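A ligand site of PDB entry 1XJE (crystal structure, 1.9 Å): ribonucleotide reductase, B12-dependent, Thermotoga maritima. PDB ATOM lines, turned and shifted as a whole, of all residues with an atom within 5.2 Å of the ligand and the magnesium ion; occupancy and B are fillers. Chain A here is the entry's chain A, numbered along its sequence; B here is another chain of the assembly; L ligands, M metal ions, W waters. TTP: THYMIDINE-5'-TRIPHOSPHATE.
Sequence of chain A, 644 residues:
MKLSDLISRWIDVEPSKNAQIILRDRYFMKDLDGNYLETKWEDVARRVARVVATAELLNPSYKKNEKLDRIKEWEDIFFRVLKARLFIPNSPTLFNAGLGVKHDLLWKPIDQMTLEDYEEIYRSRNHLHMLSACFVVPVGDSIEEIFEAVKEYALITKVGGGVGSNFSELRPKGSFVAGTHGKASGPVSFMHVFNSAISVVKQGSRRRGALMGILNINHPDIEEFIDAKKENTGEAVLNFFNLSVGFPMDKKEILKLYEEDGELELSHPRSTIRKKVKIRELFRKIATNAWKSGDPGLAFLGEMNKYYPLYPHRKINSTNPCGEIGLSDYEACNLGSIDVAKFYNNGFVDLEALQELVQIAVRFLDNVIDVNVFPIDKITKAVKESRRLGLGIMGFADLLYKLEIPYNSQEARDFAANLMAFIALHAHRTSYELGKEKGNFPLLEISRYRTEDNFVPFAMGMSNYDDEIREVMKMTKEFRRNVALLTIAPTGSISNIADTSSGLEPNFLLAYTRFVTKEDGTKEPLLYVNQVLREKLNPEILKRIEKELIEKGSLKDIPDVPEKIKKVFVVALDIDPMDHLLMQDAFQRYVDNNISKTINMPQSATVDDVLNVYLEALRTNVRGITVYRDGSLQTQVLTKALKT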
ATOM      1  N   ASP A 141      14.234   3.966  10.032  1.00  0.00           N
ATOM      2  CA  ASP A 141      13.212   2.998   9.699  1.00  0.00           C
ATOM      3  C   ASP A 141      12.347   3.388   8.480  1.00  0.00           C
ATOM      4  O   ASP A 141      11.129   3.428   8.596  1.00  0.00           O
ATOM      5  CB  ASP A 141      12.336   2.838  10.955  1.00  0.00           C
ATOM      6  CG  ASP A 141      11.444   1.617  10.938  1.00  0.00           C
ATOM      7  OD1 ASP A 141      11.744   0.550  10.395  1.00  0.00           O
ATOM      8  OD2 ASP A 141      10.364   1.743  11.520  1.00  0.00           O
ATOM      9  N   SER A 142      12.989   3.571   7.331  1.00  0.00           N
ATOM     10  CA  SER A 142      12.287   3.879   6.073  1.00  0.00           C
ATOM     11  C   SER A 142      13.125   3.383   4.896  1.00  0.00           C
ATOM     12  O   SER A 142      14.309   3.250   5.034  1.00  0.00           O
ATOM     13  CB  SER A 142      12.007   5.383   5.924  1.00  0.00           C
ATOM     14  OG  SER A 142      13.184   6.122   5.763  1.00  0.00           O
ATOM     15  N   ILE A 143      12.493   3.091   3.754  1.00  0.00           N
ATOM     16  CA  ILE A 143      13.209   2.617   2.576  1.00  0.00           C
ATOM     17  C   ILE A 143      14.221   3.689   2.139  1.00  0.00           C
ATOM     18  O   ILE A 143      15.367   3.404   1.835  1.00  0.00           O
ATOM     19  CB  ILE A 143      12.193   2.249   1.447  1.00  0.00           C
ATOM     20  CG1 ILE A 143      11.499   0.917   1.728  1.00  0.00           C
ATOM     21  CG2 ILE A 143      12.849   2.194   0.050  1.00  0.00           C
ATOM     22  CD1 ILE A 143      12.394  -0.254   2.005  1.00  0.00           C
ATOM     23  N   GLU A 144      13.800   4.946   2.178  1.00  0.00           N
ATOM     24  CA  GLU A 144      14.649   6.049   1.785  1.00  0.00           C
ATOM     25  C   GLU A 144      15.923   6.119   2.658  1.00  0.00           C
ATOM     26  O   GLU A 144      17.028   6.281   2.150  1.00  0.00           O
ATOM     27  CB  GLU A 144      13.853   7.359   1.918  1.00  0.00           C
ATOM     28  CG  GLU A 144      14.712   8.693   1.947  1.00  0.00           C
ATOM     29  CD  GLU A 144      15.348   9.041   0.617  1.00  0.00           C
ATOM     30  OE1 GLU A 144      14.728   8.750  -0.439  1.00  0.00           O
ATOM     31  OE2 GLU A 144      16.501   9.618   0.647  1.00  0.00           O
ATOM     32  N   ILE A 146      17.232   3.700   4.744  1.00  0.00           N
ATOM     33  CA  ILE A 146      17.985   2.469   4.591  1.00  0.00           C
ATOM     34  C   ILE A 146      18.921   2.592   3.380  1.00  0.00           C
ATOM     35  O   ILE A 146      20.117   2.357   3.506  1.00  0.00           O
ATOM     36  CB  ILE A 146      17.077   1.266   4.457  1.00  0.00           C
ATOM     37  CG1 ILE A 146      16.402   0.948   5.808  1.00  0.00           C
ATOM     38  CG2 ILE A 146      17.834   0.010   4.022  1.00  0.00           C
ATOM     39  CD1 ILE A 146      15.177   0.014   5.689  1.00  0.00           C
ATOM     40  N   LEU A 170      15.108  -0.316  12.833  1.00  0.00           N
ATOM     41  CA  LEU A 170      14.336  -1.056  11.859  1.00  0.00           C
ATOM     42  C   LEU A 170      13.316  -1.958  12.510  1.00  0.00           C
ATOM     43  O   LEU A 170      13.672  -2.722  13.363  1.00  0.00           O
ATOM     44  CB  LEU A 170      15.281  -1.883  10.964  1.00  0.00           C
ATOM     45  CG  LEU A 170      16.346  -1.042  10.242  1.00  0.00           C
ATOM     46  CD1 LEU A 170      17.026  -1.921   9.182  1.00  0.00           C
ATOM     47  CD2 LEU A 170      15.798   0.238   9.628  1.00  0.00           C
ATOM     48  N   ARG A 171      12.034  -1.833  12.103  1.00  0.00           N
ATOM     49  CA  ARG A 171      10.945  -2.565  12.747  1.00  0.00           C
ATOM     50  C   ARG A 171      11.085  -4.036  12.483  1.00  0.00           C
ATOM     51  O   ARG A 171      11.621  -4.437  11.430  1.00  0.00           O
ATOM     52  CB  ARG A 171       9.559  -2.073  12.342  1.00  0.00           C
ATOM     53  CG  ARG A 171       9.202  -2.135  10.837  1.00  0.00           C
ATOM     54  CD  ARG A 171       7.921  -1.352  10.490  1.00  0.00           C
ATOM     55  NE  ARG A 171       8.175   0.061  10.429  1.00  0.00           N
ATOM     56  CZ  ARG A 171       7.398   0.976   9.862  1.00  0.00           C
ATOM     57  NH1 ARG A 171       6.272   0.633   9.338  1.00  0.00           N
ATOM     58  NH2 ARG A 171       7.756   2.246   9.878  1.00  0.00           N
ATOM     59  N   PHE A 176       3.735  -4.192  10.460  1.00  0.00           N
ATOM     60  CA  PHE A 176       2.953  -3.533   9.436  1.00  0.00           C
ATOM     61  C   PHE A 176       3.727  -2.403   8.755  1.00  0.00           C
ATOM     62  O   PHE A 176       4.398  -1.595   9.406  1.00  0.00           O
ATOM     63  CB  PHE A 176       1.661  -2.975  10.072  1.00  0.00           C
ATOM     64  CG  PHE A 176       0.615  -2.534   9.056  1.00  0.00           C
ATOM     65  CD1 PHE A 176       0.164  -1.226   9.033  1.00  0.00           C
ATOM     66  CD2 PHE A 176       0.072  -3.432   8.181  1.00  0.00           C
ATOM     67  CE1 PHE A 176      -0.795  -0.826   8.135  1.00  0.00           C
ATOM     68  CE2 PHE A 176      -0.909  -3.058   7.298  1.00  0.00           C
ATOM     69  CZ  PHE A 176      -1.322  -1.738   7.252  1.00  0.00           C
ATOM     70  N   VAL A 177       3.604  -2.368   7.424  1.00  0.00           N
ATOM     71  CA  VAL A 177       4.065  -1.223   6.607  1.00  0.00           C
ATOM     72  C   VAL A 177       2.861  -0.478   6.031  1.00  0.00           C
ATOM     73  O   VAL A 177       2.247  -0.939   5.089  1.00  0.00           O
ATOM     74  CB  VAL A 177       5.010  -1.691   5.424  1.00  0.00           C
ATOM     75  CG1 VAL A 177       5.570  -0.511   4.727  1.00  0.00           C
ATOM     76  CG2 VAL A 177       6.123  -2.577   5.967  1.00  0.00           C
ATOM     77  N   ALA A 178       2.550   0.705   6.566  1.00  0.00           N
ATOM     78  CA  ALA A 178       1.306   1.392   6.169  1.00  0.00           C
ATOM     79  C   ALA A 178       1.298   1.851   4.716  1.00  0.00           C
ATOM     80  O   ALA A 178       0.245   1.826   4.074  1.00  0.00           O
ATOM     81  CB  ALA A 178       1.025   2.571   7.076  1.00  0.00           C
ATOM     82  N   GLY A 179       2.437   2.310   4.200  1.00  0.00           N
ATOM     83  CA  GLY A 179       2.480   2.828   2.844  1.00  0.00           C
ATOM     84  C   GLY A 179       2.179   1.796   1.746  1.00  0.00           C
ATOM     85  O   GLY A 179       1.816   2.166   0.628  1.00  0.00           O
ATOM     86  N   THR A 180       2.304   0.526   2.073  1.00  0.00           N
ATOM     87  CA  THR A 180       2.038  -0.535   1.121  1.00  0.00           C
ATOM     88  C   THR A 180       1.068  -1.564   1.615  1.00  0.00           C
ATOM     89  O   THR A 180       0.778  -2.486   0.903  1.00  0.00           O
ATOM     90  CB  THR A 180       3.316  -1.327   0.736  1.00  0.00           C
ATOM     91  OG1 THR A 180       3.835  -2.019   1.886  1.00  0.00           O
ATOM     92  CG2 THR A 180       4.351  -0.373   0.188  1.00  0.00           C
ATOM     93  N   LYS A 183       4.231  -6.245   5.003  1.00  0.00           N
ATOM     94  CA  LYS A 183       4.908  -6.732   6.215  1.00  0.00           C
ATOM     95  C   LYS A 183       6.416  -6.458   6.087  1.00  0.00           C
ATOM     96  O   LYS A 183       6.981  -6.704   5.045  1.00  0.00           O
ATOM     97  CB  LYS A 183       4.690  -8.221   6.357  1.00  0.00           C
ATOM     98  CG  LYS A 183       3.263  -8.608   6.746  1.00  0.00           C
ATOM     99  CD  LYS A 183       3.200 -10.088   7.026  1.00  0.00           C
ATOM    100  CE  LYS A 183       1.995 -10.791   6.351  1.00  0.00           C
ATOM    101  NZ  LYS A 183       1.892 -12.249   6.847  1.00  0.00           N
ATOM    102  N   ALA A 184       7.023  -5.944   7.137  1.00  0.00           N
ATOM    103  CA  ALA A 184       8.429  -5.541   7.114  1.00  0.00           C
ATOM    104  C   ALA A 184       9.339  -6.721   7.013  1.00  0.00           C
ATOM    105  O   ALA A 184       9.070  -7.784   7.554  1.00  0.00           O
ATOM    106  CB  ALA A 184       8.778  -4.715   8.346  1.00  0.00           C
ATOM    107  N   SER A 185      10.451  -6.529   6.310  1.00  0.00           N
ATOM    108  CA  SER A 185      11.473  -7.571   6.183  1.00  0.00           C
ATOM    109  C   SER A 185      12.282  -7.771   7.473  1.00  0.00           C
ATOM    110  O   SER A 185      12.682  -8.886   7.766  1.00  0.00           O
ATOM    111  CB  SER A 185      12.372  -7.226   4.987  1.00  0.00           C
ATOM    112  OG  SER A 185      11.662  -7.551   3.787  1.00  0.00           O
ATOM    113  N   GLY A 186      12.450  -6.714   8.277  1.00  0.00           N
ATOM    114  CA  GLY A 186      13.209  -6.796   9.537  1.00  0.00           C
ATOM    115  C   GLY A 186      14.695  -6.464   9.337  1.00  0.00           C
ATOM    116  O   GLY A 186      15.192  -6.573   8.233  1.00  0.00           O
ATOM    117  N   PHE A 190      17.639  -6.687   5.925  1.00  0.00           N
ATOM    118  CA  PHE A 190      18.315  -5.495   5.399  1.00  0.00           C
ATOM    119  C   PHE A 190      19.841  -5.553   5.519  1.00  0.00           C
ATOM    120  O   PHE A 190      20.515  -5.159   4.605  1.00  0.00           O
ATOM    121  CB  PHE A 190      17.717  -4.212   5.934  1.00  0.00           C
ATOM    122  CG  PHE A 190      16.394  -3.880   5.316  1.00  0.00           C
ATOM    123  CD1 PHE A 190      16.304  -3.532   3.988  1.00  0.00           C
ATOM    124  CD2 PHE A 190      15.225  -3.961   6.053  1.00  0.00           C
ATOM    125  CE1 PHE A 190      15.081  -3.267   3.394  1.00  0.00           C
ATOM    126  CE2 PHE A 190      14.022  -3.702   5.472  1.00  0.00           C
ATOM    127  CZ  PHE A 190      13.938  -3.351   4.151  1.00  0.00           C
ATOM    128  N   LEU B 128       2.386   8.679  -2.411  1.00  0.00           N
ATOM    129  CA  LEU B 128       2.262   7.338  -2.898  1.00  0.00           C
ATOM    130  C   LEU B 128       1.310   7.231  -4.099  1.00  0.00           C
ATOM    131  O   LEU B 128       1.073   6.134  -4.597  1.00  0.00           O
ATOM    132  CB  LEU B 128       1.701   6.485  -1.780  1.00  0.00           C
ATOM    133  CG  LEU B 128       2.502   6.465  -0.470  1.00  0.00           C
ATOM    134  CD1 LEU B 128       1.753   5.576   0.494  1.00  0.00           C
ATOM    135  CD2 LEU B 128       3.897   5.946  -0.704  1.00  0.00           C
ATOM    136  N   LYS B 158       8.746   0.202  -4.395  1.00  0.00           N
ATOM    137  CA  LYS B 158       7.806   0.421  -3.243  1.00  0.00           C
ATOM    138  C   LYS B 158       6.405   0.922  -3.654  1.00  0.00           C
ATOM    139  O   LYS B 158       5.408   0.486  -3.076  1.00  0.00           O
ATOM    140  CB  LYS B 158       8.435   1.438  -2.281  1.00  0.00           C
ATOM    141  CG  LYS B 158       7.518   1.898  -1.146  1.00  0.00           C
ATOM    142  CD  LYS B 158       8.173   2.720  -0.104  1.00  0.00           C
ATOM    143  CE  LYS B 158       7.117   3.357   0.822  1.00  0.00           C
ATOM    144  NZ  LYS B 158       7.735   4.391   1.691  1.00  0.00           N
ATOM    145  N   VAL B 200      14.087  -7.274  -1.044  1.00  0.00           N
ATOM    146  CA  VAL B 200      13.520  -6.798   0.197  1.00  0.00           C
ATOM    147  C   VAL B 200      12.550  -5.619   0.077  1.00  0.00           C
ATOM    148  O   VAL B 200      12.137  -5.059   1.128  1.00  0.00           O
ATOM    149  CB  VAL B 200      14.571  -6.394   1.255  1.00  0.00           C
ATOM    150  CG1 VAL B 200      15.375  -7.589   1.660  1.00  0.00           C
ATOM    151  CG2 VAL B 200      15.529  -5.292   0.784  1.00  0.00           C
ATOM    152  N   VAL B 201      12.197  -5.224  -1.142  1.00  0.00           N
ATOM    153  CA  VAL B 201      11.281  -4.113  -1.352  1.00  0.00           C
ATOM    154  C   VAL B 201      10.207  -4.612  -2.298  1.00  0.00           C
ATOM    155  O   VAL B 201      10.523  -5.218  -3.305  1.00  0.00           O
ATOM    156  CB  VAL B 201      11.953  -2.872  -1.974  1.00  0.00           C
ATOM    157  CG1 VAL B 201      10.971  -1.657  -2.004  1.00  0.00           C
ATOM    158  CG2 VAL B 201      13.164  -2.466  -1.204  1.00  0.00           C
ATOM    159  N   LYS B 202       8.937  -4.309  -1.979  1.00  0.00           N
ATOM    160  CA  LYS B 202       7.809  -4.586  -2.828  1.00  0.00           C
ATOM    161  C   LYS B 202       6.620  -3.690  -2.504  1.00  0.00           C
ATOM    162  O   LYS B 202       6.642  -2.962  -1.503  1.00  0.00           O
ATOM    163  CB  LYS B 202       7.384  -6.032  -2.691  1.00  0.00           C
ATOM    164  CG  LYS B 202       7.186  -6.503  -1.303  1.00  0.00           C
ATOM    165  CD  LYS B 202       6.996  -7.983  -1.353  1.00  0.00           C
ATOM    166  CE  LYS B 202       6.649  -8.539   0.003  1.00  0.00           C
ATOM    167  NZ  LYS B 202       7.151  -9.914   0.159  1.00  0.00           N
ATOM    168  N   GLN B 203       5.622  -3.699  -3.375  1.00  0.00           N
ATOM    169  CA  GLN B 203       4.392  -2.978  -3.086  1.00  0.00           C
ATOM    170  C   GLN B 203       3.497  -3.963  -2.316  1.00  0.00           C
ATOM    171  O   GLN B 203       2.509  -4.512  -2.811  1.00  0.00           O
ATOM    172  CB  GLN B 203       3.716  -2.407  -4.330  1.00  0.00           C
ATOM    173  CG  GLN B 203       2.694  -1.379  -3.938  1.00  0.00           C
ATOM    174  CD  GLN B 203       1.695  -1.023  -4.976  1.00  0.00           C
ATOM    175  OE1 GLN B 203       0.903  -0.083  -4.773  1.00  0.00           O
ATOM    176  NE2 GLN B 203       1.710  -1.701  -6.068  1.00  0.00           N
ATOM    177  N   GLY B 204       3.922  -4.221  -1.074  1.00  0.00           N
ATOM    178  CA  GLY B 204       3.245  -5.197  -0.220  1.00  0.00           C
ATOM    179  C   GLY B 204       2.892  -6.461  -0.981  1.00  0.00           C
ATOM    180  O   GLY B 204       3.651  -6.956  -1.831  1.00  0.00           O
HETATM  181  PA  TTP L   1       8.785   2.920   4.808  1.00  0.00           P
HETATM  182  O1A TTP L   1       8.924   3.972   5.817  1.00  0.00           O
HETATM  183  O2A TTP L   1       9.561   3.231   3.579  1.00  0.00           O
HETATM  184  O3A TTP L   1       7.280   2.542   4.564  1.00  0.00           O
HETATM  185  PB  TTP L   1       5.959   3.716   4.716  1.00  0.00           P
HETATM  186  O1B TTP L   1       5.267   3.670   3.408  1.00  0.00           O
HETATM  187  O2B TTP L   1       6.465   5.012   5.238  1.00  0.00           O
HETATM  188  O3B TTP L   1       5.052   3.051   5.755  1.00  0.00           O
HETATM  189  PG  TTP L   1       5.091   3.439   7.337  1.00  0.00           P
HETATM  190  O1G TTP L   1       4.373   2.371   8.069  1.00  0.00           O
HETATM  191  O2G TTP L   1       6.499   3.818   7.690  1.00  0.00           O
HETATM  192  O3G TTP L   1       4.204   4.836   7.553  1.00  0.00           O
HETATM  193  O5' TTP L   1       9.273   1.583   5.468  1.00  0.00           O
HETATM  194  C5' TTP L   1       9.203   1.307   6.809  1.00  0.00           C
HETATM  195  C4' TTP L   1       9.888   0.003   7.288  1.00  0.00           C
HETATM  196  O4' TTP L   1       9.337  -1.079   6.599  1.00  0.00           O
HETATM  197  C3' TTP L   1      11.389   0.004   7.038  1.00  0.00           C
HETATM  198  O3' TTP L   1      12.089  -0.725   8.049  1.00  0.00           O
HETATM  199  C2' TTP L   1      11.468  -0.657   5.694  1.00  0.00           C
HETATM  200  C1' TTP L   1      10.387  -1.807   5.877  1.00  0.00           C
HETATM  201  N1  TTP L   1       9.950  -2.228   4.551  1.00  0.00           N
HETATM  202  C2  TTP L   1      10.133  -3.526   4.046  1.00  0.00           C
HETATM  203  O2  TTP L   1      10.696  -4.363   4.723  1.00  0.00           O
HETATM  204  N3  TTP L   1       9.683  -3.827   2.808  1.00  0.00           N
HETATM  205  C4  TTP L   1       9.039  -2.928   2.012  1.00  0.00           C
HETATM  206  O4  TTP L   1       8.618  -3.242   0.767  1.00  0.00           O
HETATM  207  C5  TTP L   1       8.807  -1.643   2.454  1.00  0.00           C
HETATM  208  C5M TTP L   1       8.129  -0.702   1.630  1.00  0.00           C
HETATM  209  C6  TTP L   1       9.268  -1.295   3.706  1.00  0.00           C
HETATM  210 MG    MG M   1       7.604   5.100   6.807  1.00  0.00          MG
HETATM  211  O   HOH W   1      10.864   5.626   2.333  1.00  0.00           O
HETATM  212  O   HOH W   2       8.891   5.261   8.618  1.00  0.00           O
HETATM  213  O   HOH W   3       9.729  -6.438   2.103  1.00  0.00           O
HETATM  214  O   HOH W   4       5.856  -3.684   1.273  1.00  0.00           O
HETATM  215  O   HOH W   5       5.803   6.026   3.046  1.00  0.00           O
HETATM  216  O   HOH W   6       8.629   6.123   3.849  1.00  0.00           O
HETATM  217  O   HOH W   7       6.135   6.656   7.922  1.00  0.00           O
HETATM  218  O   HOH W   8      12.232  -3.803   8.781  1.00  0.00           O
HETATM  219  O   HOH W   9       8.407   6.660   6.319  1.00  0.00           O
HETATM  220  O   HOH W  10       6.886  -5.740   2.446  1.00  0.00           O
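An oxygen (O3') of the ligand lies within hydrogen-bond range of the side-chain carboxylate (OD1) of Asp 141, at 2.7 Å. N of Ser 185 lies within hydrogen-bond range of O2 of the ligand (2.7 Å). O2 of the ligand lies close to OG of Ser 185. NH1 of Arg 171 is in salt-bridge range of O1G of the ligand, 2.9 Å away. The side-chain amino group (NZ) of Lys 158 of chain B lies within salt-bridge range of an oxygen (O2A) of the ligand. N of Ala 178 lies within hydrogen-bond range of O1G of the ligand (2.9 Å). An oxygen (O2A) of the ligand lies within hydrogen-bond range of the backbone NH (N) of Ile 143, at 2.9 Å. N of Lys 202 of chain B is in hydrogen-bond range of O4 of the ligand. O3B of the ligand sits at hydrogen-bond distance from N of Gly 179 (3.1 Å). The backbone carbonyl oxygen (O) of Val 200 of chain B is in hydrogen-bond range of a nitrogen (N3) of the ligand (3.2 Å).
NE of Arg 171 is in salt-bridge range of OD2 of Asp 141 (3.0 Å). The backbone carbonyl oxygen (O) of Phe 176 is in hydrogen-bond range of the guanidinium group (NH1) of Arg 171 (2.9 Å).
Ser 142 touches the ligand. Ile 146 touches the ligand. Val 177 touches the ligand. Ala 184 touches the ligand (CA to O2, 3.5 Å). Phe 190 touches the ligand (CZ to O2, 3.4 Å). Val 201 of chain B touches the ligand. Hydrophobic or aromatic side chains within 4 Å of the ligand: Ile 143, Ile 146, Val 177, Ala 178, Phe 190 and Val 201 of chain B. 15 residues have an atom within 4 Å of the ligand: Asp 141, Ser 142, Ile 143, Ile 146, Arg 171, Val 177, Ala 178, Gly 179, Ala 184, Ser 185, Phe 190, Lys 158 of chain B, Val 200 of chain B, Val 201 of chain B and Lys 202 of chain B. The nearest printed residue that does not touch the ligand is Thr 180 (4.1 Å).
No residue comes within 4 Å of the magnesium ion. The nearest printed residue that does not touch the magnesium ion is Arg 171 (4.2 Å).
The magnesium ion is bound by water W9, 1.8 Å away. The magnesium ion is bound by O2G of the ligand, at 1.9 Å. The magnesium ion is bound by an oxygen (O2B) of the ligand (1.9 Å). An oxygen (O1A) of the ligand binds the magnesium ion. The magnesium ion is bound by water W2, at 2.2 Å. The magnesium ion is bound by water W7, at 2.4 Å. The magnesium ion has six donor atoms within binding distance.
Water W2 bridges the backbone carbonyl oxygen of Asp 141 (2.9 Å) and the guanidinium group of Arg 171 (3.5 Å). Water W5 lies within hydrogen-bond range of an oxygen (O1B) of the ligand (2.4 Å) and the side-chain amino group (NZ) of Lys 158 of chain B (2.9 Å). Water W6 bridges NZ of Lys 158 of chain B and O2A of the ligand. Water W4 lies within hydrogen-bond range of the side-chain hydroxyl of Thr 180, an oxygen (O4) of the ligand, the backbone carbonyl oxygen of Lys 202 of chain B and the backbone NH of Gly 204 of chain B. Water W8 lies within hydrogen-bond range of O of Arg 171 (2.8 Å), N of Gly 186 (3.0 Å) and O3' of the ligand (3.2 Å). Water W10 lies within hydrogen-bond range of O of Lys 183 and N3 of the ligand.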
